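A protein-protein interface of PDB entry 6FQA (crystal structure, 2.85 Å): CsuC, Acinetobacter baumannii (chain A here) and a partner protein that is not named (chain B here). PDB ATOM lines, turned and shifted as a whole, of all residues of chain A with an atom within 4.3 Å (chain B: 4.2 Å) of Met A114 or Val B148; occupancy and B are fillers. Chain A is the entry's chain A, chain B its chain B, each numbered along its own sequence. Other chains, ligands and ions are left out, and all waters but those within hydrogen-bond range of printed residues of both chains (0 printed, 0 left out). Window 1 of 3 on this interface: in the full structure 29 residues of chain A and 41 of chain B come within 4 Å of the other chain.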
ATOM      1  N   ASP A  93       9.260   3.841 -21.375  1.00  0.00           N
ATOM      2  CA  ASP A  93      10.556   3.393 -20.865  1.00  0.00           C
ATOM      3  C   ASP A  93      11.013   4.323 -19.756  1.00  0.00           C
ATOM      4  O   ASP A  93      11.281   5.498 -20.013  1.00  0.00           O
ATOM      5  CB  ASP A  93      11.596   3.358 -21.984  1.00  0.00           C
ATOM      6  CG  ASP A  93      11.762   1.977 -22.590  1.00  0.00           C
ATOM      7  OD1 ASP A  93      11.798   1.009 -21.818  1.00  0.00           O
ATOM      8  OD2 ASP A  93      11.870   1.850 -23.824  1.00  0.00           O
ATOM      9  N   GLU A  94      11.110   3.800 -18.532  1.00  0.00           N
ATOM     10  CA  GLU A  94      11.513   4.595 -17.369  1.00  0.00           C
ATOM     11  C   GLU A  94      13.028   4.765 -17.376  1.00  0.00           C
ATOM     12  O   GLU A  94      13.761   3.791 -17.188  1.00  0.00           O
ATOM     13  CB  GLU A  94      11.043   3.917 -16.086  1.00  0.00           C
ATOM     14  CG  GLU A  94      11.494   4.564 -14.786  1.00  0.00           C
ATOM     15  CD  GLU A  94      11.624   3.546 -13.660  1.00  0.00           C
ATOM     16  OE1 GLU A  94      12.585   2.733 -13.712  1.00  0.00           O
ATOM     17  OE2 GLU A  94      10.759   3.549 -12.749  1.00  0.00           O
ATOM     18  N   PHE A 112      16.890  -2.932 -11.506  1.00  0.00           N
ATOM     19  CA  PHE A 112      15.790  -3.103 -12.447  1.00  0.00           C
ATOM     20  C   PHE A 112      15.440  -1.802 -13.145  1.00  0.00           C
ATOM     21  O   PHE A 112      15.246  -0.772 -12.492  1.00  0.00           O
ATOM     22  CB  PHE A 112      14.550  -3.652 -11.745  1.00  0.00           C
ATOM     23  CG  PHE A 112      14.734  -5.022 -11.196  1.00  0.00           C
ATOM     24  CD1 PHE A 112      14.963  -6.084 -12.039  1.00  0.00           C
ATOM     25  CD2 PHE A 112      14.692  -5.245  -9.832  1.00  0.00           C
ATOM     26  CE1 PHE A 112      15.139  -7.345 -11.529  1.00  0.00           C
ATOM     27  CE2 PHE A 112      14.867  -6.498  -9.312  1.00  0.00           C
ATOM     28  CZ  PHE A 112      15.084  -7.554 -10.158  1.00  0.00           C
ATOM     29  N   GLN A 113      15.327  -1.869 -14.465  1.00  0.00           N
ATOM     30  CA  GLN A 113      14.768  -0.800 -15.278  1.00  0.00           C
ATOM     31  C   GLN A 113      13.404  -1.250 -15.787  1.00  0.00           C
ATOM     32  O   GLN A 113      13.285  -2.325 -16.379  1.00  0.00           O
ATOM     33  CB  GLN A 113      15.704  -0.473 -16.442  1.00  0.00           C
ATOM     34  CG  GLN A 113      15.284   0.715 -17.276  1.00  0.00           C
ATOM     35  CD  GLN A 113      16.321   1.075 -18.319  1.00  0.00           C
ATOM     36  OE1 GLN A 113      17.512   0.798 -18.152  1.00  0.00           O
ATOM     37  NE2 GLN A 113      15.871   1.691 -19.406  1.00  0.00           N
ATOM     38  N   MET A 114      12.379  -0.448 -15.554  1.00  0.00           N
ATOM     39  CA  MET A 114      11.038  -0.851 -15.936  1.00  0.00           C
ATOM     40  C   MET A 114      10.704  -0.407 -17.353  1.00  0.00           C
ATOM     41  O   MET A 114      11.233   0.586 -17.864  1.00  0.00           O
ATOM     42  CB  MET A 114      10.001  -0.283 -14.977  1.00  0.00           C
ATOM     43  CG  MET A 114      10.184  -0.696 -13.529  1.00  0.00           C
ATOM     44  SD  MET A 114      10.313  -2.473 -13.303  1.00  0.00           S
ATOM     45  CE  MET A 114       8.837  -3.014 -14.159  1.00  0.00           C
ATOM     46  N   ARG A 115       9.810  -1.165 -17.988  1.00  0.00           N
ATOM     47  CA  ARG A 115       9.260  -0.836 -19.294  1.00  0.00           C
ATOM     48  C   ARG A 115       7.811  -1.282 -19.343  1.00  0.00           C
ATOM     49  O   ARG A 115       7.516  -2.446 -19.069  1.00  0.00           O
ATOM     50  CB  ARG A 115      10.026  -1.503 -20.418  1.00  0.00           C
ATOM     51  CG  ARG A 115       9.279  -1.333 -21.705  1.00  0.00           C
ATOM     52  CD  ARG A 115       9.944  -2.040 -22.846  1.00  0.00           C
ATOM     53  NE  ARG A 115      11.057  -1.270 -23.374  1.00  0.00           N
ATOM     54  CZ  ARG A 115      11.626  -1.527 -24.538  1.00  0.00           C
ATOM     55  NH1 ARG A 115      11.158  -2.523 -25.277  1.00  0.00           N
ATOM     56  NH2 ARG A 115      12.646  -0.793 -24.962  1.00  0.00           N
ATOM     57  N   TYR A 116       6.914  -0.370 -19.711  1.00  0.00           N
ATOM     58  CA  TYR A 116       5.478  -0.633 -19.716  1.00  0.00           C
ATOM     59  C   TYR A 116       4.933  -0.525 -21.132  1.00  0.00           C
ATOM     60  O   TYR A 116       5.257   0.406 -21.869  1.00  0.00           O
ATOM     61  CB  TYR A 116       4.741   0.336 -18.777  1.00  0.00           C
ATOM     62  CG  TYR A 116       5.366   0.326 -17.414  1.00  0.00           C
ATOM     63  CD1 TYR A 116       5.225  -0.779 -16.577  1.00  0.00           C
ATOM     64  CD2 TYR A 116       6.148   1.387 -16.982  1.00  0.00           C
ATOM     65  CE1 TYR A 116       5.825  -0.818 -15.335  1.00  0.00           C
ATOM     66  CE2 TYR A 116       6.745   1.371 -15.735  1.00  0.00           C
ATOM     67  CZ  TYR A 116       6.586   0.262 -14.915  1.00  0.00           C
ATOM     68  OH  TYR A 116       7.188   0.239 -13.673  1.00  0.00           O
ATOM     69  N   ILE B  56       7.531  -4.773  -6.964  1.00  0.00           N
ATOM     70  CA  ILE B  56       6.733  -4.413  -8.133  1.00  0.00           C
ATOM     71  C   ILE B  56       5.361  -5.072  -8.056  1.00  0.00           C
ATOM     72  O   ILE B  56       5.243  -6.226  -7.625  1.00  0.00           O
ATOM     73  CB  ILE B  56       7.484  -4.837  -9.409  1.00  0.00           C
ATOM     74  CG1 ILE B  56       8.854  -4.172  -9.443  1.00  0.00           C
ATOM     75  CG2 ILE B  56       6.670  -4.562 -10.641  1.00  0.00           C
ATOM     76  CD1 ILE B  56       9.771  -4.732 -10.469  1.00  0.00           C
ATOM     77  N   VAL B  70       4.738 -10.292 -18.028  1.00  0.00           N
ATOM     78  CA  VAL B  70       6.018  -9.768 -17.563  1.00  0.00           C
ATOM     79  C   VAL B  70       7.134 -10.574 -18.216  1.00  0.00           C
ATOM     80  O   VAL B  70       7.090 -11.807 -18.212  1.00  0.00           O
ATOM     81  CB  VAL B  70       6.132  -9.829 -16.026  1.00  0.00           C
ATOM     82  CG1 VAL B  70       7.517  -9.495 -15.607  1.00  0.00           C
ATOM     83  CG2 VAL B  70       5.137  -8.883 -15.362  1.00  0.00           C
ATOM     84  N   ALA B  71       8.122  -9.879 -18.785  1.00  0.00           N
ATOM     85  CA  ALA B  71       9.294 -10.495 -19.397  1.00  0.00           C
ATOM     86  C   ALA B  71      10.560  -9.832 -18.877  1.00  0.00           C
ATOM     87  O   ALA B  71      10.585  -8.615 -18.675  1.00  0.00           O
ATOM     88  CB  ALA B  71       9.248 -10.386 -20.926  1.00  0.00           C
ATOM     89  N   LEU B 146      18.690  -5.274 -15.196  1.00  0.00           N
ATOM     90  CA  LEU B 146      17.700  -6.080 -15.909  1.00  0.00           C
ATOM     91  C   LEU B 146      16.543  -5.228 -16.418  1.00  0.00           C
ATOM     92  O   LEU B 146      16.025  -4.365 -15.698  1.00  0.00           O
ATOM     93  CB  LEU B 146      17.136  -7.192 -15.023  1.00  0.00           C
ATOM     94  CG  LEU B 146      17.907  -8.505 -14.848  1.00  0.00           C
ATOM     95  CD1 LEU B 146      17.210  -9.397 -13.827  1.00  0.00           C
ATOM     96  CD2 LEU B 146      18.076  -9.237 -16.186  1.00  0.00           C
ATOM     97  N   LEU B 147      16.121  -5.498 -17.652  1.00  0.00           N
ATOM     98  CA  LEU B 147      14.966  -4.825 -18.232  1.00  0.00           C
ATOM     99  C   LEU B 147      13.720  -5.668 -17.973  1.00  0.00           C
ATOM    100  O   LEU B 147      13.620  -6.808 -18.436  1.00  0.00           O
ATOM    101  CB  LEU B 147      15.148  -4.580 -19.732  1.00  0.00           C
ATOM    102  CG  LEU B 147      13.914  -3.863 -20.296  1.00  0.00           C
ATOM    103  CD1 LEU B 147      13.725  -2.507 -19.611  1.00  0.00           C
ATOM    104  CD2 LEU B 147      13.905  -3.716 -21.806  1.00  0.00           C
ATOM    105  N   VAL B 148      12.775  -5.105 -17.242  1.00  0.00           N
ATOM    106  CA  VAL B 148      11.548  -5.790 -16.869  1.00  0.00           C
ATOM    107  C   VAL B 148      10.430  -5.154 -17.675  1.00  0.00           C
ATOM    108  O   VAL B 148      10.088  -3.988 -17.445  1.00  0.00           O
ATOM    109  CB  VAL B 148      11.266  -5.681 -15.362  1.00  0.00           C
ATOM    110  CG1 VAL B 148       9.946  -6.324 -15.042  1.00  0.00           C
ATOM    111  CG2 VAL B 148      12.388  -6.306 -14.537  1.00  0.00           C
ATOM    112  N   THR B 149       9.871  -5.900 -18.630  1.00  0.00           N
ATOM    113  CA  THR B 149       8.765  -5.421 -19.455  1.00  0.00           C
ATOM    114  C   THR B 149       7.435  -5.947 -18.923  1.00  0.00           C
ATOM    115  O   THR B 149       7.258  -7.160 -18.771  1.00  0.00           O
ATOM    116  CB  THR B 149       8.932  -5.843 -20.913  1.00  0.00           C
ATOM    117  OG1 THR B 149      10.284  -5.626 -21.335  1.00  0.00           O
ATOM    118  CG2 THR B 149       7.978  -5.056 -21.798  1.00  0.00           C
ATOM    119  N   VAL B 150       6.502  -5.036 -18.661  1.00  0.00           N
ATOM    120  CA  VAL B 150       5.135  -5.365 -18.260  1.00  0.00           C
ATOM    121  C   VAL B 150       4.229  -5.009 -19.426  1.00  0.00           C
ATOM    122  O   VAL B 150       4.197  -3.850 -19.859  1.00  0.00           O
ATOM    123  CB  VAL B 150       4.723  -4.608 -16.986  1.00  0.00           C
ATOM    124  CG1 VAL B 150       3.310  -4.884 -16.643  1.00  0.00           C
ATOM    125  CG2 VAL B 150       5.622  -4.977 -15.828  1.00  0.00           C
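Printed residues of chain A that touch a printed residue of chain B: Phe A112, Gln A113, Met A114, Arg A115 and Tyr A116. Hydrophobic or aromatic side chains of chain A that line the printed part of chain B: Phe A112, Met A114 and Tyr A116. Printed residues of chain B that touch a printed residue of chain A: Ile B56, Leu B146, Leu B147, Val B148, Thr B149 and Val B150.
Among the printed residues, merely in contact across the chains: Phe A112 with Leu B146 (3.5 Å), Phe A112 with Val B148 (3.6 Å), Gln A113 with Leu B147 (3.3 Å), Met A114 with Ile B56 (3.7 Å), Met A114 with Val B148 (3.6 Å), Arg A115 with Leu B147 (3.9 Å), Arg A115 with Thr B149 (3.2 Å) and Tyr A116 with Val B150 (3.5 Å).
The backbone NH of Gln A113 sits at hydrogen-bond distance from the backbone carbonyl oxygen of Leu B146 (2.9 Å). The backbone carbonyl oxygen (O) of Gln A113 sits at hydrogen-bond distance from the backbone NH (N) of Val B148, at 3.0 Å. O of Val B148 is in hydrogen-bond range of N of Arg A115, 2.9 Å away. The backbone carbonyl oxygen (O) of Arg A115 lies within hydrogen-bond range of the backbone NH (N) of Val B150.
The side-chain carboxylate (OD1) of Asp A93 is in salt-bridge range of the guanidinium group (NE) of Arg A115, at 2.9 Å. The backbone NH (N) of Glu A94 sits at hydrogen-bond distance from the backbone carbonyl oxygen (O) of Met A114, 3.3 Å away. The backbone carbonyl oxygen (O) of Ala B71 is in hydrogen-bond range of the backbone NH (N) of Thr B149 (2.8 Å).
Of the printed residues of chain B, Met A114 touches Ile B56 (3.7 Å) and Val B148 (3.6 Å). Of the printed residues of chain B, Arg A115 touches Leu B147, Val B148, Thr B149 and Val B150. Of the printed residues of chain A, Thr B149 touches Arg A115 (3.2 Å). Printed residues of chain B within 4 Å of Phe A112: Leu B146 and Val B148. Of the printed residues of chain A, Ile B56 touches Met A114. Of the printed residues of chain A, Leu B146 touches Phe A112 and Gln A113. The nearest residue of chain B that does not touch Met A114 is Val B150 (4.1 Å). The nearest printed residue of chain A that does not touch Val B148 is Tyr A116 (5.3 Å).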
